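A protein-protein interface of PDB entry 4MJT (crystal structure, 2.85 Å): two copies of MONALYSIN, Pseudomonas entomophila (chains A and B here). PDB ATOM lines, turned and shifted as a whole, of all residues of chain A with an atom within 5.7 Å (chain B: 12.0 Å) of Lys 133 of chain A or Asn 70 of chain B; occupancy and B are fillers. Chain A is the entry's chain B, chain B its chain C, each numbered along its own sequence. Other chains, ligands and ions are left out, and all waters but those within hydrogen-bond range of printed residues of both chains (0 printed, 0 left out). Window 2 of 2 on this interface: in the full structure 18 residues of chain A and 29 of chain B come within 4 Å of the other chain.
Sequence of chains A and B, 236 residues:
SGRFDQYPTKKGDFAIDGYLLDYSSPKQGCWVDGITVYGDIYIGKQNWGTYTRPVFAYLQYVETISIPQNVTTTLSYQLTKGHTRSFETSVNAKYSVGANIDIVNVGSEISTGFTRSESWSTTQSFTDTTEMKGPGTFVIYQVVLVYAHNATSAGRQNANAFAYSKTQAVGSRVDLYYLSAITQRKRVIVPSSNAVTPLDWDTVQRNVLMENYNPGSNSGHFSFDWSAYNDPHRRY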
ATOM      1  N   ILE A  67      41.661   9.969  25.473  1.00  0.00           N
ATOM      2  CA  ILE A  67      40.756   9.141  26.274  1.00  0.00           C
ATOM      3  C   ILE A  67      41.408   7.744  26.303  1.00  0.00           C
ATOM      4  O   ILE A  67      41.385   7.052  25.285  1.00  0.00           O
ATOM      5  CB  ILE A  67      39.287   9.113  25.741  1.00  0.00           C
ATOM      6  CG1 ILE A  67      38.769  10.525  25.371  1.00  0.00           C
ATOM      7  CG2 ILE A  67      38.357   8.436  26.764  1.00  0.00           C
ATOM      8  CD1 ILE A  67      37.611  10.560  24.364  1.00  0.00           C
ATOM      9  N   GLN A  69      40.608   4.891  27.934  1.00  0.00           N
ATOM     10  CA  GLN A  69      39.734   3.727  28.149  1.00  0.00           C
ATOM     11  C   GLN A  69      38.392   3.767  27.422  1.00  0.00           C
ATOM     12  O   GLN A  69      37.968   4.832  26.976  1.00  0.00           O
ATOM     13  CB  GLN A  69      39.499   3.535  29.651  1.00  0.00           C
ATOM     14  CG  GLN A  69      40.741   3.051  30.375  1.00  0.00           C
ATOM     15  CD  GLN A  69      40.630   3.120  31.868  1.00  0.00           C
ATOM     16  OE1 GLN A  69      39.951   3.980  32.444  1.00  0.00           O
ATOM     17  NE2 GLN A  69      41.359   2.242  32.528  1.00  0.00           N
ATOM     18  N   VAL A  71      35.384   4.347  27.898  1.00  0.00           N
ATOM     19  CA  VAL A  71      34.549   5.130  28.799  1.00  0.00           C
ATOM     20  C   VAL A  71      33.888   6.254  28.007  1.00  0.00           C
ATOM     21  O   VAL A  71      34.574   6.967  27.273  1.00  0.00           O
ATOM     22  CB  VAL A  71      35.428   5.695  29.955  1.00  0.00           C
ATOM     23  CG1 VAL A  71      34.686   6.738  30.777  1.00  0.00           C
ATOM     24  CG2 VAL A  71      35.970   4.586  30.851  1.00  0.00           C
ATOM     25  N   THR A  72      32.566   6.417  28.165  1.00  0.00           N
ATOM     26  CA  THR A  72      31.810   7.502  27.541  1.00  0.00           C
ATOM     27  C   THR A  72      31.917   8.718  28.476  1.00  0.00           C
ATOM     28  O   THR A  72      31.631   8.615  29.674  1.00  0.00           O
ATOM     29  CB  THR A  72      30.364   7.071  27.230  1.00  0.00           C
ATOM     30  OG1 THR A  72      30.390   5.866  26.457  1.00  0.00           O
ATOM     31  CG2 THR A  72      29.581   8.145  26.479  1.00  0.00           C
ATOM     32  N   THR A  73      32.380   9.851  27.930  1.00  0.00           N
ATOM     33  CA  THR A  73      32.575  11.096  28.678  1.00  0.00           C
ATOM     34  C   THR A  73      32.080  12.321  27.898  1.00  0.00           C
ATOM     35  O   THR A  73      31.787  12.219  26.706  1.00  0.00           O
ATOM     36  CB  THR A  73      34.034  11.229  29.171  1.00  0.00           C
ATOM     37  OG1 THR A  73      34.146  12.362  30.034  1.00  0.00           O
ATOM     38  CG2 THR A  73      35.046  11.317  28.032  1.00  0.00           C
ATOM     39  N   GLU A 131      29.887  14.742  23.397  1.00  0.00           N
ATOM     40  CA  GLU A 131      29.882  13.432  24.038  1.00  0.00           C
ATOM     41  C   GLU A 131      30.831  12.532  23.251  1.00  0.00           C
ATOM     42  O   GLU A 131      30.667  12.357  22.041  1.00  0.00           O
ATOM     43  CB  GLU A 131      28.458  12.863  24.061  1.00  0.00           C
ATOM     44  CG  GLU A 131      27.669  13.222  25.307  1.00  0.00           C
ATOM     45  CD  GLU A 131      27.779  12.202  26.422  1.00  0.00           C
ATOM     46  OE1 GLU A 131      27.186  11.107  26.286  1.00  0.00           O
ATOM     47  OE2 GLU A 131      28.445  12.501  27.439  1.00  0.00           O
ATOM     48  N   MET A 132      31.866  12.014  23.927  1.00  0.00           N
ATOM     49  CA  MET A 132      32.906  11.184  23.304  1.00  0.00           C
ATOM     50  C   MET A 132      33.187   9.901  24.070  1.00  0.00           C
ATOM     51  O   MET A 132      33.260   9.922  25.300  1.00  0.00           O
ATOM     52  CB  MET A 132      34.219  11.985  23.207  1.00  0.00           C
ATOM     53  CG  MET A 132      34.151  13.173  22.269  1.00  0.00           C
ATOM     54  SD  MET A 132      34.371  12.728  20.532  1.00  0.00           S
ATOM     55  CE  MET A 132      36.050  12.330  20.531  1.00  0.00           C
ATOM     56  N   LYS A 133      33.403   8.795  23.341  1.00  0.00           N
ATOM     57  CA  LYS A 133      33.762   7.514  23.960  1.00  0.00           C
ATOM     58  C   LYS A 133      35.117   7.025  23.475  1.00  0.00           C
ATOM     59  O   LYS A 133      35.413   7.119  22.292  1.00  0.00           O
ATOM     60  CB  LYS A 133      32.665   6.437  23.825  1.00  0.00           C
ATOM     61  CG  LYS A 133      32.242   6.073  22.404  1.00  0.00           C
ATOM     62  CD  LYS A 133      31.365   4.808  22.358  1.00  0.00           C
ATOM     63  CE  LYS A 133      29.935   5.012  22.814  1.00  0.00           C
ATOM     64  NZ  LYS A 133      29.086   3.819  22.548  1.00  0.00           N
ATOM     65  N   GLY A 134      35.946   6.555  24.398  1.00  0.00           N
ATOM     66  CA  GLY A 134      37.275   6.054  24.067  1.00  0.00           C
ATOM     67  C   GLY A 134      37.312   4.549  23.863  1.00  0.00           C
ATOM     68  O   GLY A 134      36.252   3.914  23.785  1.00  0.00           O
ATOM     69  N   PRO A 135      38.514   3.922  23.788  1.00  0.00           N
ATOM     70  CA  PRO A 135      39.859   4.520  23.860  1.00  0.00           C
ATOM     71  C   PRO A 135      40.289   5.166  22.545  1.00  0.00           C
ATOM     72  O   PRO A 135      39.876   4.725  21.473  1.00  0.00           O
ATOM     73  CB  PRO A 135      40.738   3.324  24.231  1.00  0.00           C
ATOM     74  CG  PRO A 135      40.071   2.163  23.556  1.00  0.00           C
ATOM     75  CD  PRO A 135      38.589   2.458  23.601  1.00  0.00           C
ATOM     76  N   PHE A 138      42.141  12.156  19.770  1.00  0.00           N
ATOM     77  CA  PHE A 138      41.343  12.927  18.814  1.00  0.00           C
ATOM     78  C   PHE A 138      41.847  14.332  18.645  1.00  0.00           C
ATOM     79  O   PHE A 138      42.449  14.885  19.564  1.00  0.00           O
ATOM     80  CB  PHE A 138      39.870  12.948  19.240  1.00  0.00           C
ATOM     81  CG  PHE A 138      39.301  11.576  19.507  1.00  0.00           C
ATOM     82  CD1 PHE A 138      39.411  10.991  20.765  1.00  0.00           C
ATOM     83  CD2 PHE A 138      38.669  10.859  18.496  1.00  0.00           C
ATOM     84  CE1 PHE A 138      38.911   9.715  21.001  1.00  0.00           C
ATOM     85  CE2 PHE A 138      38.158   9.586  18.740  1.00  0.00           C
ATOM     86  CZ  PHE A 138      38.283   9.024  19.990  1.00  0.00           C
ATOM     87  N   SER B  66      28.599  16.997  12.139  1.00  0.00           N
ATOM     88  CA  SER B  66      29.537  15.881  12.166  1.00  0.00           C
ATOM     89  C   SER B  66      29.539  15.189  13.532  1.00  0.00           C
ATOM     90  O   SER B  66      29.852  15.824  14.547  1.00  0.00           O
ATOM     91  CB  SER B  66      30.937  16.343  11.785  1.00  0.00           C
ATOM     92  OG  SER B  66      31.802  15.241  11.571  1.00  0.00           O
ATOM     93  N   ILE B  67      29.143  13.897  13.559  1.00  0.00           N
ATOM     94  CA  ILE B  67      29.144  13.055  14.760  1.00  0.00           C
ATOM     95  C   ILE B  67      30.130  11.913  14.450  1.00  0.00           C
ATOM     96  O   ILE B  67      29.796  11.040  13.648  1.00  0.00           O
ATOM     97  CB  ILE B  67      27.732  12.541  15.169  1.00  0.00           C
ATOM     98  CG1 ILE B  67      26.662  13.653  15.106  1.00  0.00           C
ATOM     99  CG2 ILE B  67      27.789  11.890  16.565  1.00  0.00           C
ATOM    100  CD1 ILE B  67      25.209  13.158  14.924  1.00  0.00           C
ATOM    101  N   PRO B  68      31.368  11.927  14.996  1.00  0.00           N
ATOM    102  CA  PRO B  68      32.342  10.889  14.607  1.00  0.00           C
ATOM    103  C   PRO B  68      32.180   9.505  15.251  1.00  0.00           C
ATOM    104  O   PRO B  68      32.832   8.560  14.794  1.00  0.00           O
ATOM    105  CB  PRO B  68      33.692  11.518  14.968  1.00  0.00           C
ATOM    106  CG  PRO B  68      33.390  12.453  16.068  1.00  0.00           C
ATOM    107  CD  PRO B  68      31.965  12.919  15.913  1.00  0.00           C
ATOM    108  N   GLN B  69      31.349   9.368  16.303  1.00  0.00           N
ATOM    109  CA  GLN B  69      31.197   8.086  17.012  1.00  0.00           C
ATOM    110  C   GLN B  69      29.760   7.617  17.194  1.00  0.00           C
ATOM    111  O   GLN B  69      28.832   8.415  17.056  1.00  0.00           O
ATOM    112  CB  GLN B  69      31.880   8.167  18.384  1.00  0.00           C
ATOM    113  CG  GLN B  69      33.385   8.219  18.290  1.00  0.00           C
ATOM    114  CD  GLN B  69      34.042   8.613  19.576  1.00  0.00           C
ATOM    115  OE1 GLN B  69      33.536   9.426  20.361  1.00  0.00           O
ATOM    116  NE2 GLN B  69      35.221   8.074  19.786  1.00  0.00           N
ATOM    117  N   ASN B  70      29.586   6.326  17.561  1.00  0.00           N
ATOM    118  CA  ASN B  70      28.288   5.703  17.843  1.00  0.00           C
ATOM    119  C   ASN B  70      27.793   6.170  19.225  1.00  0.00           C
ATOM    120  O   ASN B  70      27.711   5.397  20.184  1.00  0.00           O
ATOM    121  CB  ASN B  70      28.361   4.166  17.710  1.00  0.00           C
ATOM    122  CG  ASN B  70      29.456   3.505  18.518  1.00  0.00           C
ATOM    123  OD1 ASN B  70      30.641   3.865  18.435  1.00  0.00           O
ATOM    124  ND2 ASN B  70      29.079   2.514  19.318  1.00  0.00           N
ATOM    125  N   VAL B  71      27.495   7.475  19.310  1.00  0.00           N
ATOM    126  CA  VAL B  71      27.070   8.190  20.506  1.00  0.00           C
ATOM    127  C   VAL B  71      25.755   8.901  20.212  1.00  0.00           C
ATOM    128  O   VAL B  71      25.649   9.593  19.201  1.00  0.00           O
ATOM    129  CB  VAL B  71      28.181   9.196  20.928  1.00  0.00           C
ATOM    130  CG1 VAL B  71      27.695  10.165  21.993  1.00  0.00           C
ATOM    131  CG2 VAL B  71      29.444   8.479  21.397  1.00  0.00           C
ATOM    132  N   THR B  72      24.765   8.745  21.102  1.00  0.00           N
ATOM    133  CA  THR B  72      23.476   9.430  20.997  1.00  0.00           C
ATOM    134  C   THR B  72      23.651  10.796  21.660  1.00  0.00           C
ATOM    135  O   THR B  72      24.108  10.876  22.801  1.00  0.00           O
ATOM    136  CB  THR B  72      22.333   8.578  21.589  1.00  0.00           C
ATOM    137  OG1 THR B  72      22.338   7.286  20.969  1.00  0.00           O
ATOM    138  CG2 THR B  72      20.959   9.226  21.410  1.00  0.00           C
ATOM    139  N   THR B  73      23.335  11.866  20.924  1.00  0.00           N
ATOM    140  CA  THR B  73      23.467  13.247  21.392  1.00  0.00           C
ATOM    141  C   THR B  73      22.245  14.107  21.002  1.00  0.00           C
ATOM    142  O   THR B  73      21.419  13.698  20.184  1.00  0.00           O
ATOM    143  CB  THR B  73      24.819  13.856  20.943  1.00  0.00           C
ATOM    144  OG1 THR B  73      24.976  15.136  21.560  1.00  0.00           O
ATOM    145  CG2 THR B  73      24.960  13.980  19.415  1.00  0.00           C
ATOM    146  N   THR B  74      22.134  15.291  21.614  1.00  0.00           N
ATOM    147  CA  THR B  74      21.057  16.236  21.342  1.00  0.00           C
ATOM    148  C   THR B  74      21.636  17.427  20.566  1.00  0.00           C
ATOM    149  O   THR B  74      22.591  18.065  21.021  1.00  0.00           O
ATOM    150  CB  THR B  74      20.266  16.560  22.618  1.00  0.00           C
ATOM    151  OG1 THR B  74      19.161  17.393  22.282  1.00  0.00           O
ATOM    152  CG2 THR B  74      21.117  17.168  23.739  1.00  0.00           C
ATOM    153  N   GLU B 131      17.312  14.867  18.495  1.00  0.00           N
ATOM    154  CA  GLU B 131      18.091  13.786  19.090  1.00  0.00           C
ATOM    155  C   GLU B 131      18.710  12.996  17.939  1.00  0.00           C
ATOM    156  O   GLU B 131      17.983  12.507  17.071  1.00  0.00           O
ATOM    157  CB  GLU B 131      17.191  12.904  19.967  1.00  0.00           C
ATOM    158  CG  GLU B 131      17.161  13.299  21.432  1.00  0.00           C
ATOM    159  CD  GLU B 131      18.194  12.589  22.286  1.00  0.00           C
ATOM    160  OE1 GLU B 131      18.032  11.371  22.539  1.00  0.00           O
ATOM    161  OE2 GLU B 131      19.159  13.259  22.719  1.00  0.00           O
ATOM    162  N   MET B 132      20.049  12.929  17.896  1.00  0.00           N
ATOM    163  CA  MET B 132      20.792  12.276  16.817  1.00  0.00           C
ATOM    164  C   MET B 132      21.861  11.312  17.311  1.00  0.00           C
ATOM    165  O   MET B 132      22.561  11.616  18.275  1.00  0.00           O
ATOM    166  CB  MET B 132      21.464  13.340  15.932  1.00  0.00           C
ATOM    167  CG  MET B 132      20.488  14.198  15.160  1.00  0.00           C
ATOM    168  SD  MET B 132      19.914  13.415  13.646  1.00  0.00           S
ATOM    169  CE  MET B 132      21.351  13.547  12.680  1.00  0.00           C
ATOM    170  N   LYS B 133      22.024  10.173  16.620  1.00  0.00           N
ATOM    171  CA  LYS B 133      23.066   9.206  16.954  1.00  0.00           C
ATOM    172  C   LYS B 133      24.018   9.006  15.786  1.00  0.00           C
ATOM    173  O   LYS B 133      23.579   8.918  14.649  1.00  0.00           O
ATOM    174  CB  LYS B 133      22.503   7.875  17.495  1.00  0.00           C
ATOM    175  CG  LYS B 133      21.551   7.104  16.570  1.00  0.00           C
ATOM    176  CD  LYS B 133      21.289   5.662  17.050  1.00  0.00           C
ATOM    177  CE  LYS B 133      20.395   5.554  18.271  1.00  0.00           C
ATOM    178  NZ  LYS B 133      20.043   4.144  18.584  1.00  0.00           N
ATOM    179  N   GLY B 134      25.315   8.969  16.072  1.00  0.00           N
ATOM    180  CA  GLY B 134      26.328   8.768  15.043  1.00  0.00           C
ATOM    181  C   GLY B 134      26.761   7.319  14.901  1.00  0.00           C
ATOM    182  O   GLY B 134      26.117   6.429  15.466  1.00  0.00           O
ATOM    183  N   PRO B 135      27.855   7.022  14.157  1.00  0.00           N
ATOM    184  CA  PRO B 135      28.727   7.952  13.414  1.00  0.00           C
ATOM    185  C   PRO B 135      28.131   8.395  12.083  1.00  0.00           C
ATOM    186  O   PRO B 135      27.392   7.640  11.461  1.00  0.00           O
ATOM    187  CB  PRO B 135      30.011   7.136  13.233  1.00  0.00           C
ATOM    188  CG  PRO B 135      29.528   5.723  13.110  1.00  0.00           C
ATOM    189  CD  PRO B 135      28.312   5.623  14.005  1.00  0.00           C
ATOM    190  N   GLY B 136      28.448   9.615  11.668  1.00  0.00           N
ATOM    191  CA  GLY B 136      27.973  10.161  10.403  1.00  0.00           C
ATOM    192  C   GLY B 136      28.018  11.667  10.269  1.00  0.00           C
ATOM    193  O   GLY B 136      28.194  12.387  11.252  1.00  0.00           O
ATOM    194  N   THR B 137      27.867  12.138   9.023  1.00  0.00           N
ATOM    195  CA  THR B 137      27.802  13.550   8.655  1.00  0.00           C
ATOM    196  C   THR B 137      26.400  13.795   8.102  1.00  0.00           C
ATOM    197  O   THR B 137      25.882  12.970   7.349  1.00  0.00           O
ATOM    198  CB  THR B 137      28.961  13.945   7.738  1.00  0.00           C
ATOM    199  OG1 THR B 137      30.190  13.587   8.379  1.00  0.00           O
ATOM    200  CG2 THR B 137      28.986  15.439   7.435  1.00  0.00           C
ATOM    201  N   PHE B 138      25.759  14.884   8.537  1.00  0.00           N
ATOM    202  CA  PHE B 138      24.376  15.201   8.178  1.00  0.00           C
ATOM    203  C   PHE B 138      24.220  16.630   7.727  1.00  0.00           C
ATOM    204  O   PHE B 138      24.987  17.492   8.143  1.00  0.00           O
ATOM    205  CB  PHE B 138      23.436  14.926   9.373  1.00  0.00           C
ATOM    206  CG  PHE B 138      23.579  13.541   9.962  1.00  0.00           C
ATOM    207  CD1 PHE B 138      24.531  13.282  10.951  1.00  0.00           C
ATOM    208  CD2 PHE B 138      22.798  12.485   9.496  1.00  0.00           C
ATOM    209  CE1 PHE B 138      24.693  11.995  11.467  1.00  0.00           C
ATOM    210  CE2 PHE B 138      22.952  11.206  10.019  1.00  0.00           C
ATOM    211  CZ  PHE B 138      23.900  10.968  11.003  1.00  0.00           C
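OE1 of Gln 69 of chain B sits close to SD of Met 132 of chain A. The backbone carbonyl oxygen (O) of Lys 133 of chain A is in hydrogen-bond range of the side-chain amide nitrogen (NE2) of Gln 69 of chain B (2.7 Å). The side-chain amino group (NZ) of Lys 133 of chain A is in hydrogen-bond range of the backbone carbonyl oxygen (O) of Asn 70 of chain B, 3.2 Å away.
The backbone NH (N) of Thr 73 of chain A sits at hydrogen-bond distance from the backbone carbonyl oxygen (O) of Met 132 of chain A, 2.8 Å away. The backbone carbonyl oxygen (O) of Val 71 of chain B lies within hydrogen-bond range of the backbone NH (N) of Gly 134 of chain B.
Among the printed residues, pairs that only touch across the chains: Glu 131 of chain A with Val 71 of chain B (3.5 Å), Lys 133 of chain A with Val 71 of chain B (3.8 Å) and Phe 138 of chain A with Gln 69 of chain B (3.2 Å).
Lys 133 of chain A touches three residues of chain B. Of the printed residues of chain A, Asn 70 of chain B touches Lys 133 (3.2 Å). No residue of chain B comes within 4 Å of Ile 67 of chain A. No residue of chain B comes within 4 Å of Thr 73 of chain A. Met 132 of chain A touches one residue of chain B. No residue of chain B comes within 4 Å of Gly 134 of chain A. Pro 135 of chain A touches none of the printed residues of chain B. Printed residues of chain A within 4 Å of Gln 69 of chain B: Met 132 (3.4 Å), Lys 133 (2.7 Å) and Phe 138 (3.2 Å). Of the printed residues of chain B, Phe 138 of chain A touches Gln 69 (3.2 Å). Of the printed residues of chain A, Val 71 of chain B touches Glu 131 and Lys 133. Ile 67 of chain B touches none of the printed residues of chain A. The nearest residue of chain B that does not touch Lys 133 of chain A is Thr 72 of chain B (6.6 Å). The nearest printed residue of chain A that does not touch Asn 70 of chain B is Thr 72 of chain A (6.8 Å). The nearest printed residue of chain A that does not touch Val 71 of chain B is Met 132 of chain A (4.8 Å).
Hydrophobic or aromatic side chains of chain A that line the printed part of chain B: Met 132 and Phe 138. Along chain A the printed residues that touch a printed residue of chain B span positions 131 to 138. Along chain B the printed residues that touch a printed residue of chain A span positions 69 to 71. Among the printed residues, 6 pairs touch across the chains. Among the printed residues, no Asp or Glu carboxylate lies within 4 Å of a Lys or Arg side-chain nitrogen of the other chain.
Glu 131 of chain A touches Val 71 of chain B, but with the chains exchanged Val 71 of chain A does not touch Glu 131 of chain B (17.1 Å). Met 132 of chain A touches Gln 69 of chain B, but with the chains exchanged Gln 69 of chain A does not touch Met 132 of chain B (19.0 Å). Lys 133 of chain A touches Val 71 of chain B, but with the chains exchanged Val 71 of chain A does not touch Lys 133 of chain B (15.6 Å). Phe 138 of chain A touches Gln 69 of chain B, but with the chains exchanged Gln 69 of chain A does not touch Phe 138 of chain B (21.6 Å). 11 positions are printed for both chains.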
